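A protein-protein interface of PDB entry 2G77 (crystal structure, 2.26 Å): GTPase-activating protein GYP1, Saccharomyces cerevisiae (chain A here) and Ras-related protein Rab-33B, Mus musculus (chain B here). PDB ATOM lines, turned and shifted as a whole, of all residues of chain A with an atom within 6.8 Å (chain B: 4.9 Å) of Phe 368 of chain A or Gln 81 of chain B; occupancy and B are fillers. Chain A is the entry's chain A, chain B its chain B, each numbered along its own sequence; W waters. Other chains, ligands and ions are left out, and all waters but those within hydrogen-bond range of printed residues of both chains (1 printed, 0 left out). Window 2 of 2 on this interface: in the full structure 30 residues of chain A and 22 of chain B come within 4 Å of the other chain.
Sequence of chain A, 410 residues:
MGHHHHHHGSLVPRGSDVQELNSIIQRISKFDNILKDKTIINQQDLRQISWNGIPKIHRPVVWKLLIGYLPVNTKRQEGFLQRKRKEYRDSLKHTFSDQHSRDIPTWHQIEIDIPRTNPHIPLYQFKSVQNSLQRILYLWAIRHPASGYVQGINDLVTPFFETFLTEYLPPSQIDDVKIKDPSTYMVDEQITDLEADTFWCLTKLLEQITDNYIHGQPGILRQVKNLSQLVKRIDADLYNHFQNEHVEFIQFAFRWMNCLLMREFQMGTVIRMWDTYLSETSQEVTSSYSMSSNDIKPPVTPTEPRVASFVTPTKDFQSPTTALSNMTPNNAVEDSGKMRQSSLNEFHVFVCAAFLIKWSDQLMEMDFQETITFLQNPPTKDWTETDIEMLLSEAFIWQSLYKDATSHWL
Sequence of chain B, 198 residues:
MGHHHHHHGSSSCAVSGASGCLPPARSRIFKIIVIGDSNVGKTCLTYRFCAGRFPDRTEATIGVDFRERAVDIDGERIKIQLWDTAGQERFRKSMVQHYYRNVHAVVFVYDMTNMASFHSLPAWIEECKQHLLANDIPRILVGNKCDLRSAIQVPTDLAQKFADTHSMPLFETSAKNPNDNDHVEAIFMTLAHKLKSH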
ATOM      1  N   HIS A 241      16.244  15.003 -17.308  1.00  0.00           N
ATOM      2  CA  HIS A 241      16.674  15.900 -18.413  1.00  0.00           C
ATOM      3  C   HIS A 241      16.126  17.300 -18.242  1.00  0.00           C
ATOM      4  O   HIS A 241      16.807  18.262 -18.619  1.00  0.00           O
ATOM      5  CB  HIS A 241      16.233  15.374 -19.774  1.00  0.00           C
ATOM      6  CG  HIS A 241      16.618  16.252 -20.928  1.00  0.00           C
ATOM      7  ND1 HIS A 241      17.924  16.423 -21.329  1.00  0.00           N
ATOM      8  CD2 HIS A 241      15.865  16.980 -21.794  1.00  0.00           C
ATOM      9  CE1 HIS A 241      17.969  17.219 -22.389  1.00  0.00           C
ATOM     10  NE2 HIS A 241      16.731  17.593 -22.679  1.00  0.00           N
ATOM     11  N   PHE A 242      14.890  17.406 -17.729  1.00  0.00           N
ATOM     12  CA  PHE A 242      14.170  18.703 -17.559  1.00  0.00           C
ATOM     13  C   PHE A 242      14.860  19.503 -16.464  1.00  0.00           C
ATOM     14  O   PHE A 242      15.095  20.686 -16.650  1.00  0.00           O
ATOM     15  CB  PHE A 242      12.711  18.497 -17.110  1.00  0.00           C
ATOM     16  CG  PHE A 242      11.697  18.332 -18.238  1.00  0.00           C
ATOM     17  CD1 PHE A 242      12.079  18.219 -19.564  1.00  0.00           C
ATOM     18  CD2 PHE A 242      10.331  18.262 -17.934  1.00  0.00           C
ATOM     19  CE1 PHE A 242      11.124  18.072 -20.568  1.00  0.00           C
ATOM     20  CE2 PHE A 242       9.368  18.108 -18.954  1.00  0.00           C
ATOM     21  CZ  PHE A 242       9.769  17.997 -20.255  1.00  0.00           C
ATOM     22  N   GLU A 245      18.059  21.028 -17.518  1.00  0.00           N
ATOM     23  CA  GLU A 245      17.949  22.156 -18.458  1.00  0.00           C
ATOM     24  C   GLU A 245      17.129  23.282 -17.852  1.00  0.00           C
ATOM     25  O   GLU A 245      16.918  24.297 -18.528  1.00  0.00           O
ATOM     26  CB  GLU A 245      17.293  21.724 -19.771  1.00  0.00           C
ATOM     27  CG  GLU A 245      17.900  20.527 -20.450  1.00  0.00           C
ATOM     28  CD  GLU A 245      19.330  20.776 -20.871  1.00  0.00           C
ATOM     29  OE1 GLU A 245      19.586  21.801 -21.523  1.00  0.00           O
ATOM     30  OE2 GLU A 245      20.199  19.931 -20.550  1.00  0.00           O
ATOM     31  N   HIS A 246      16.669  23.083 -16.611  1.00  0.00           N
ATOM     32  CA  HIS A 246      15.867  24.050 -15.859  1.00  0.00           C
ATOM     33  C   HIS A 246      14.459  24.268 -16.456  1.00  0.00           C
ATOM     34  O   HIS A 246      13.845  25.303 -16.288  1.00  0.00           O
ATOM     35  CB  HIS A 246      16.669  25.336 -15.604  1.00  0.00           C
ATOM     36  CG  HIS A 246      18.037  25.064 -15.041  1.00  0.00           C
ATOM     37  ND1 HIS A 246      18.230  24.458 -13.809  1.00  0.00           N
ATOM     38  CD2 HIS A 246      19.273  25.224 -15.578  1.00  0.00           C
ATOM     39  CE1 HIS A 246      19.526  24.296 -13.597  1.00  0.00           C
ATOM     40  NE2 HIS A 246      20.179  24.742 -14.659  1.00  0.00           N
ATOM     41  N   VAL A 247      13.972  23.236 -17.145  1.00  0.00           N
ATOM     42  CA  VAL A 247      12.587  23.128 -17.611  1.00  0.00           C
ATOM     43  C   VAL A 247      11.695  22.888 -16.425  1.00  0.00           C
ATOM     44  O   VAL A 247      11.880  21.913 -15.628  1.00  0.00           O
ATOM     45  CB  VAL A 247      12.366  22.063 -18.724  1.00  0.00           C
ATOM     46  CG1 VAL A 247      10.854  21.967 -19.043  1.00  0.00           C
ATOM     47  CG2 VAL A 247      13.171  22.436 -19.994  1.00  0.00           C
ATOM     48  N   GLU A 248      10.809  23.859 -16.242  1.00  0.00           N
ATOM     49  CA  GLU A 248       9.780  23.782 -15.223  1.00  0.00           C
ATOM     50  C   GLU A 248       8.430  23.393 -15.851  1.00  0.00           C
ATOM     51  O   GLU A 248       8.016  23.938 -16.870  1.00  0.00           O
ATOM     52  CB  GLU A 248       9.661  25.126 -14.471  1.00  0.00           C
ATOM     53  CG  GLU A 248      10.849  25.482 -13.534  1.00  0.00           C
ATOM     54  CD  GLU A 248      10.796  26.981 -13.109  1.00  0.00           C
ATOM     55  OE1 GLU A 248       9.809  27.368 -12.377  1.00  0.00           O
ATOM     56  OE2 GLU A 248      11.722  27.763 -13.520  1.00  0.00           O
ATOM     57  N   GLN A 251       6.043  26.121 -17.004  1.00  0.00           N
ATOM     58  CA  GLN A 251       6.242  26.943 -18.197  1.00  0.00           C
ATOM     59  C   GLN A 251       5.454  26.470 -19.428  1.00  0.00           C
ATOM     60  O   GLN A 251       5.384  27.193 -20.406  1.00  0.00           O
ATOM     61  CB  GLN A 251       7.732  27.106 -18.519  1.00  0.00           C
ATOM     62  CG  GLN A 251       8.519  27.589 -17.287  1.00  0.00           C
ATOM     63  CD  GLN A 251      10.026  27.367 -17.328  1.00  0.00           C
ATOM     64  OE1 GLN A 251      10.522  26.271 -17.697  1.00  0.00           O
ATOM     65  NE2 GLN A 251      10.785  28.420 -16.920  1.00  0.00           N
ATOM     66  N   MET A 366      16.766  17.974 -26.436  1.00  0.00           N
ATOM     67  CA  MET A 366      16.452  19.397 -26.584  1.00  0.00           C
ATOM     68  C   MET A 366      16.981  20.199 -25.417  1.00  0.00           C
ATOM     69  O   MET A 366      16.973  19.722 -24.278  1.00  0.00           O
ATOM     70  CB  MET A 366      14.933  19.598 -26.724  1.00  0.00           C
ATOM     71  CG  MET A 366      14.358  19.273 -28.118  1.00  0.00           C
ATOM     72  SD  MET A 366      12.572  19.567 -28.036  1.00  0.00           S
ATOM     73  CE  MET A 366      12.025  19.034 -29.677  1.00  0.00           C
ATOM     74  N   ASP A 367      17.465  21.407 -25.704  1.00  0.00           N
ATOM     75  CA  ASP A 367      17.825  22.333 -24.641  1.00  0.00           C
ATOM     76  C   ASP A 367      16.581  23.100 -24.183  1.00  0.00           C
ATOM     77  O   ASP A 367      15.461  22.805 -24.631  1.00  0.00           O
ATOM     78  CB  ASP A 367      18.954  23.277 -25.049  1.00  0.00           C
ATOM     79  CG  ASP A 367      18.560  24.250 -26.160  1.00  0.00           C
ATOM     80  OD1 ASP A 367      17.382  24.342 -26.574  1.00  0.00           O
ATOM     81  OD2 ASP A 367      19.470  24.936 -26.648  1.00  0.00           O
ATOM     82  N   PHE A 368      16.764  24.038 -23.265  1.00  0.00           N
ATOM     83  CA  PHE A 368      15.646  24.700 -22.636  1.00  0.00           C
ATOM     84  C   PHE A 368      14.823  25.445 -23.674  1.00  0.00           C
ATOM     85  O   PHE A 368      13.624  25.275 -23.701  1.00  0.00           O
ATOM     86  CB  PHE A 368      16.108  25.627 -21.515  1.00  0.00           C
ATOM     87  CG  PHE A 368      15.024  26.546 -20.984  1.00  0.00           C
ATOM     88  CD1 PHE A 368      14.311  26.213 -19.836  1.00  0.00           C
ATOM     89  CD2 PHE A 368      14.748  27.745 -21.620  1.00  0.00           C
ATOM     90  CE1 PHE A 368      13.291  27.073 -19.370  1.00  0.00           C
ATOM     91  CE2 PHE A 368      13.766  28.594 -21.158  1.00  0.00           C
ATOM     92  CZ  PHE A 368      13.062  28.286 -20.026  1.00  0.00           C
ATOM     93  N   GLN A 369      15.421  26.232 -24.554  1.00  0.00           N
ATOM     94  CA  GLN A 369      14.554  27.034 -25.435  1.00  0.00           C
ATOM     95  C   GLN A 369      13.792  26.157 -26.387  1.00  0.00           C
ATOM     96  O   GLN A 369      12.662  26.478 -26.699  1.00  0.00           O
ATOM     97  CB  GLN A 369      15.265  28.165 -26.180  1.00  0.00           C
ATOM     98  CG  GLN A 369      16.095  27.797 -27.335  1.00  0.00           C
ATOM     99  CD  GLN A 369      15.376  27.668 -28.713  1.00  0.00           C
ATOM    100  OE1 GLN A 369      14.207  28.028 -28.892  1.00  0.00           O
ATOM    101  NE2 GLN A 369      16.111  27.125 -29.686  1.00  0.00           N
ATOM    102  N   GLU A 370      14.419  25.054 -26.827  1.00  0.00           N
ATOM    103  CA  GLU A 370      13.789  24.078 -27.743  1.00  0.00           C
ATOM    104  C   GLU A 370      12.623  23.369 -27.053  1.00  0.00           C
ATOM    105  O   GLU A 370      11.596  23.163 -27.624  1.00  0.00           O
ATOM    106  CB  GLU A 370      14.817  23.036 -28.283  1.00  0.00           C
ATOM    107  CG  GLU A 370      15.814  23.613 -29.331  1.00  0.00           C
ATOM    108  CD  GLU A 370      17.052  22.721 -29.634  1.00  0.00           C
ATOM    109  OE1 GLU A 370      17.531  21.952 -28.716  1.00  0.00           O
ATOM    110  OE2 GLU A 370      17.558  22.845 -30.807  1.00  0.00           O
ATOM    111  N   THR A 371      12.806  22.975 -25.821  1.00  0.00           N
ATOM    112  CA  THR A 371      11.770  22.299 -25.097  1.00  0.00           C
ATOM    113  C   THR A 371      10.529  23.235 -24.984  1.00  0.00           C
ATOM    114  O   THR A 371       9.418  22.821 -25.295  1.00  0.00           O
ATOM    115  CB  THR A 371      12.332  21.923 -23.756  1.00  0.00           C
ATOM    116  OG1 THR A 371      13.455  21.082 -23.994  1.00  0.00           O
ATOM    117  CG2 THR A 371      11.330  21.197 -22.843  1.00  0.00           C
ATOM    118  N   ILE A 372      10.734  24.497 -24.624  1.00  0.00           N
ATOM    119  CA  ILE A 372       9.617  25.373 -24.255  1.00  0.00           C
ATOM    120  C   ILE A 372       8.841  25.747 -25.535  1.00  0.00           C
ATOM    121  O   ILE A 372       7.603  25.646 -25.572  1.00  0.00           O
ATOM    122  CB  ILE A 372      10.048  26.600 -23.362  1.00  0.00           C
ATOM    123  CG1 ILE A 372      10.763  26.163 -22.048  1.00  0.00           C
ATOM    124  CG2 ILE A 372       8.850  27.508 -23.074  1.00  0.00           C
ATOM    125  CD1 ILE A 372       9.944  25.235 -21.111  1.00  0.00           C
ATOM    126  N   THR A 373       9.588  26.018 -26.590  1.00  0.00           N
ATOM    127  CA  THR A 373       9.040  26.339 -27.893  1.00  0.00           C
ATOM    128  C   THR A 373       8.199  25.204 -28.436  1.00  0.00           C
ATOM    129  O   THR A 373       7.104  25.439 -28.996  1.00  0.00           O
ATOM    130  CB  THR A 373      10.168  26.660 -28.922  1.00  0.00           C
ATOM    131  OG1 THR A 373      10.891  27.809 -28.453  1.00  0.00           O
ATOM    132  CG2 THR A 373       9.605  26.913 -30.390  1.00  0.00           C
ATOM    133  N   ILE B  29      22.494  34.443 -22.737  1.00  0.00           N
ATOM    134  CA  ILE B  29      21.037  34.482 -22.897  1.00  0.00           C
ATOM    135  C   ILE B  29      20.509  35.489 -21.903  1.00  0.00           C
ATOM    136  O   ILE B  29      20.868  35.447 -20.727  1.00  0.00           O
ATOM    137  CB  ILE B  29      20.360  33.133 -22.567  1.00  0.00           C
ATOM    138  CG1 ILE B  29      20.781  32.035 -23.543  1.00  0.00           C
ATOM    139  CG2 ILE B  29      18.837  33.306 -22.497  1.00  0.00           C
ATOM    140  CD1 ILE B  29      20.755  30.650 -22.900  1.00  0.00           C
ATOM    141  N   PHE B  30      19.662  36.388 -22.386  1.00  0.00           N
ATOM    142  CA  PHE B  30      18.998  37.356 -21.535  1.00  0.00           C
ATOM    143  C   PHE B  30      17.488  37.147 -21.571  1.00  0.00           C
ATOM    144  O   PHE B  30      16.880  37.083 -22.631  1.00  0.00           O
ATOM    145  CB  PHE B  30      19.343  38.755 -21.993  1.00  0.00           C
ATOM    146  CG  PHE B  30      20.795  39.078 -21.870  1.00  0.00           C
ATOM    147  CD1 PHE B  30      21.623  39.050 -22.993  1.00  0.00           C
ATOM    148  CD2 PHE B  30      21.351  39.412 -20.621  1.00  0.00           C
ATOM    149  CE1 PHE B  30      22.990  39.376 -22.890  1.00  0.00           C
ATOM    150  CE2 PHE B  30      22.718  39.724 -20.495  1.00  0.00           C
ATOM    151  CZ  PHE B  30      23.539  39.704 -21.633  1.00  0.00           C
ATOM    152  N   LYS B  31      16.921  37.011 -20.381  1.00  0.00           N
ATOM    153  CA  LYS B  31      15.498  36.846 -20.163  1.00  0.00           C
ATOM    154  C   LYS B  31      14.808  38.200 -19.983  1.00  0.00           C
ATOM    155  O   LYS B  31      15.075  38.934 -19.036  1.00  0.00           O
ATOM    156  CB  LYS B  31      15.289  35.966 -18.938  1.00  0.00           C
ATOM    157  CG  LYS B  31      13.858  35.913 -18.416  1.00  0.00           C
ATOM    158  CD  LYS B  31      13.716  34.836 -17.345  1.00  0.00           C
ATOM    159  CE  LYS B  31      12.255  34.433 -17.128  1.00  0.00           C
ATOM    160  NZ  LYS B  31      12.175  33.279 -16.171  1.00  0.00           N
ATOM    161  N   ILE B  32      13.922  38.510 -20.915  1.00  0.00           N
ATOM    162  CA  ILE B  32      13.103  39.714 -20.852  1.00  0.00           C
ATOM    163  C   ILE B  32      11.613  39.355 -20.788  1.00  0.00           C
ATOM    164  O   ILE B  32      11.115  38.592 -21.624  1.00  0.00           O
ATOM    165  CB  ILE B  32      13.292  40.610 -22.131  1.00  0.00           C
ATOM    166  CG1 ILE B  32      14.776  40.918 -22.399  1.00  0.00           C
ATOM    167  CG2 ILE B  32      12.446  41.908 -22.011  1.00  0.00           C
ATOM    168  CD1 ILE B  32      14.988  41.984 -23.501  1.00  0.00           C
ATOM    169  N   PHE B  66       6.531  31.930 -24.796  1.00  0.00           N
ATOM    170  CA  PHE B  66       7.992  32.004 -24.884  1.00  0.00           C
ATOM    171  C   PHE B  66       8.380  32.165 -26.338  1.00  0.00           C
ATOM    172  O   PHE B  66       7.749  31.591 -27.218  1.00  0.00           O
ATOM    173  CB  PHE B  66       8.620  30.752 -24.275  1.00  0.00           C
ATOM    174  CG  PHE B  66      10.139  30.656 -24.450  1.00  0.00           C
ATOM    175  CD1 PHE B  66      11.004  31.281 -23.547  1.00  0.00           C
ATOM    176  CD2 PHE B  66      10.696  29.915 -25.505  1.00  0.00           C
ATOM    177  CE1 PHE B  66      12.411  31.197 -23.687  1.00  0.00           C
ATOM    178  CE2 PHE B  66      12.104  29.833 -25.664  1.00  0.00           C
ATOM    179  CZ  PHE B  66      12.957  30.484 -24.745  1.00  0.00           C
ATOM    180  N   ARG B  67       9.338  33.027 -26.579  1.00  0.00           N
ATOM    181  CA  ARG B  67       9.852  33.347 -27.908  1.00  0.00           C
ATOM    182  C   ARG B  67      11.321  33.716 -27.761  1.00  0.00           C
ATOM    183  O   ARG B  67      11.701  34.368 -26.792  1.00  0.00           O
ATOM    184  CB  ARG B  67       9.094  34.521 -28.540  1.00  0.00           C
ATOM    185  CG  ARG B  67       7.896  34.083 -29.390  1.00  0.00           C
ATOM    186  CD  ARG B  67       7.002  35.290 -29.845  1.00  0.00           C
ATOM    187  NE  ARG B  67       5.584  35.175 -29.449  1.00  0.00           N
ATOM    188  CZ  ARG B  67       5.110  35.268 -28.196  1.00  0.00           C
ATOM    189  NH1 ARG B  67       5.945  35.435 -27.157  1.00  0.00           N
ATOM    190  NH2 ARG B  67       3.792  35.179 -27.967  1.00  0.00           N
ATOM    191  N   GLU B  68      12.137  33.263 -28.711  1.00  0.00           N
ATOM    192  CA  GLU B  68      13.577  33.583 -28.736  1.00  0.00           C
ATOM    193  C   GLU B  68      14.037  34.391 -29.970  1.00  0.00           C
ATOM    194  O   GLU B  68      13.624  34.153 -31.103  1.00  0.00           O
ATOM    195  CB  GLU B  68      14.489  32.361 -28.501  1.00  0.00           C
ATOM    196  CG  GLU B  68      15.921  32.810 -27.997  1.00  0.00           C
ATOM    197  CD  GLU B  68      16.876  31.668 -27.671  1.00  0.00           C
ATOM    198  OE1 GLU B  68      17.182  31.457 -26.469  1.00  0.00           O
ATOM    199  OE2 GLU B  68      17.349  31.004 -28.622  1.00  0.00           O
ATOM    200  N   LYS B  79      21.421  35.883 -27.045  1.00  0.00           N
ATOM    201  CA  LYS B  79      20.083  35.312 -27.180  1.00  0.00           C
ATOM    202  C   LYS B  79      19.074  36.015 -26.274  1.00  0.00           C
ATOM    203  O   LYS B  79      19.242  36.081 -25.058  1.00  0.00           O
ATOM    204  CB  LYS B  79      20.135  33.791 -26.967  1.00  0.00           C
ATOM    205  CG  LYS B  79      20.522  33.080 -28.284  1.00  0.00           C
ATOM    206  CD  LYS B  79      21.215  31.737 -28.070  1.00  0.00           C
ATOM    207  CE  LYS B  79      21.679  31.164 -29.398  1.00  0.00           C
ATOM    208  NZ  LYS B  79      22.003  29.702 -29.260  1.00  0.00           N
ATOM    209  N   ILE B  80      18.035  36.569 -26.878  1.00  0.00           N
ATOM    210  CA  ILE B  80      16.985  37.262 -26.113  1.00  0.00           C
ATOM    211  C   ILE B  80      15.808  36.336 -25.999  1.00  0.00           C
ATOM    212  O   ILE B  80      15.162  36.026 -26.983  1.00  0.00           O
ATOM    213  CB  ILE B  80      16.451  38.577 -26.783  1.00  0.00           C
ATOM    214  CG1 ILE B  80      17.591  39.454 -27.327  1.00  0.00           C
ATOM    215  CG2 ILE B  80      15.494  39.339 -25.819  1.00  0.00           C
ATOM    216  CD1 ILE B  80      18.297  40.313 -26.308  1.00  0.00           C
ATOM    217  N   GLN B  81      15.538  35.920 -24.773  1.00  0.00           N
ATOM    218  CA  GLN B  81      14.352  35.137 -24.466  1.00  0.00           C
ATOM    219  C   GLN B  81      13.245  36.062 -23.920  1.00  0.00           C
ATOM    220  O   GLN B  81      13.393  36.655 -22.844  1.00  0.00           O
ATOM    221  CB  GLN B  81      14.715  33.978 -23.520  1.00  0.00           C
ATOM    222  CG  GLN B  81      15.506  32.940 -24.275  1.00  0.00           C
ATOM    223  CD  GLN B  81      15.993  31.775 -23.425  1.00  0.00           C
ATOM    224  OE1 GLN B  81      15.812  31.749 -22.214  1.00  0.00           O
ATOM    225  NE2 GLN B  81      16.630  30.797 -24.077  1.00  0.00           N
ATOM    226  N   LEU B  82      12.179  36.198 -24.719  1.00  0.00           N
ATOM    227  CA  LEU B  82      11.010  37.030 -24.416  1.00  0.00           C
ATOM    228  C   LEU B  82       9.853  36.225 -23.794  1.00  0.00           C
ATOM    229  O   LEU B  82       9.363  35.276 -24.374  1.00  0.00           O
ATOM    230  CB  LEU B  82      10.542  37.738 -25.688  1.00  0.00           C
ATOM    231  CG  LEU B  82      11.502  38.840 -26.144  1.00  0.00           C
ATOM    232  CD1 LEU B  82      11.247  39.296 -27.600  1.00  0.00           C
ATOM    233  CD2 LEU B  82      11.465  40.023 -25.148  1.00  0.00           C
ATOM    234  N   TRP B  83       9.466  36.582 -22.578  1.00  0.00           N
ATOM    235  CA  TRP B  83       8.349  36.000 -21.898  1.00  0.00           C
ATOM    236  C   TRP B  83       7.156  36.980 -22.005  1.00  0.00           C
ATOM    237  O   TRP B  83       7.121  37.992 -21.327  1.00  0.00           O
ATOM    238  CB  TRP B  83       8.732  35.680 -20.448  1.00  0.00           C
ATOM    239  CG  TRP B  83       9.801  34.633 -20.412  1.00  0.00           C
ATOM    240  CD1 TRP B  83      11.165  34.823 -20.570  1.00  0.00           C
ATOM    241  CD2 TRP B  83       9.611  33.214 -20.298  1.00  0.00           C
ATOM    242  NE1 TRP B  83      11.819  33.622 -20.513  1.00  0.00           N
ATOM    243  CE2 TRP B  83      10.900  32.614 -20.352  1.00  0.00           C
ATOM    244  CE3 TRP B  83       8.480  32.387 -20.141  1.00  0.00           C
ATOM    245  CZ2 TRP B  83      11.085  31.226 -20.242  1.00  0.00           C
ATOM    246  CZ3 TRP B  83       8.671  30.998 -20.027  1.00  0.00           C
ATOM    247  CH2 TRP B  83       9.960  30.443 -20.071  1.00  0.00           C
HETATM  248  O   HOH W   1      18.073  27.937 -24.035  1.00  0.00           O
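OE1 of Gln 251 of chain A is in hydrogen-bond range of N of Glu 248 of chain A (2.8 Å).
The backbone carbonyl oxygen of Gln 369 of chain A sits at hydrogen-bond distance from the side-chain hydroxyl of Thr 373 of chain A (2.8 Å).
N of Gln 81 of chain B is in hydrogen-bond range of O of Phe 30 of chain B (2.8 Å).
O of Gln 81 of chain B is in hydrogen-bond range of N of Ile 32 of chain B (2.7 Å).
The backbone carbonyl oxygen (O) of Ile 32 of chain B is in hydrogen-bond range of the backbone NH (N) of Trp 83 of chain B (2.8 Å).
The side-chain carboxylate (OE1) of Glu 68 of chain B is in hydrogen-bond range of the side-chain amide nitrogen (NE2) of Gln 81 of chain B (2.5 Å).
Gln 251 of chain A touches Trp 83 of chain B.
CE1 of Phe 66 of chain B touches CE2 of Phe 368 of chain A, at 3.9 Å.
Phe 368 of chain A touches Gln 81 of chain B (CE2 to OE1, 3.9 Å).
Trp 83 of chain B touches Phe 368 of chain A (CZ2 to CZ, 3.5 Å).
CE2 of Phe 66 of chain B touches O of Gln 369 of chain A, 3.6 Å away.
Gln 369 of chain A touches Glu 68 of chain B.
Gln 369 of chain A touches Gln 81 of chain B.
Phe 66 of chain B touches Ile 372 of chain A.
Phe 66 of chain B touches Thr 373 of chain A.
Phe 368 of chain A touches three residues of chain B.
Of chain A, only Phe 368 (3.9 Å) and Gln 369 (3.6 Å) come within 4 Å of Gln 81 of chain B.
Of the printed residues of chain A, Phe 66 of chain B touches Phe 368 (3.9 Å), Gln 369 (3.6 Å), Ile 372 (3.5 Å) and Thr 373 (3.6 Å).
Of the printed residues of chain A, Glu 68 of chain B touches Gln 369.
Of the printed residues of chain B, Ile 372 of chain A touches Phe 66 (3.5 Å).
Of the printed residues of chain B, Gln 251 of chain A touches Trp 83 (3.8 Å).
Ile 29 of chain B touches none of the printed residues of chain A.
Lys 79 of chain B touches none of the printed residues of chain A.
The nearest printed residue of chain B that does not touch Ile 372 of chain A is Trp 83 of chain B (4.3 Å).
Of the 12 printed residues of chain B, 4 touch a printed residue of chain A.
Hydrophobic or aromatic side chains of chain B within 4 Å of the printed part of chain A: Phe 66 and Trp 83.
Of the 15 printed residues of chain A, 5 touch a printed residue of chain B.
Printed residues of chain A that touch a printed residue of chain B: Gln 251, Phe 368, Gln 369, Ile 372 and Thr 373.
Hydrophobic or aromatic side chains of chain A within 4 Å of the printed part of chain B: Phe 368 and Ile 372.
Among the printed residues, no Asp or Glu carboxylate lies within 4 Å of a Lys or Arg side-chain nitrogen of the other chain.
Water W1 bridges the backbone NH (N) of Gln 369 of chain A (3.2 Å) and the side-chain amide nitrogen (NE2) of Gln 81 of chain B (3.2 Å).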
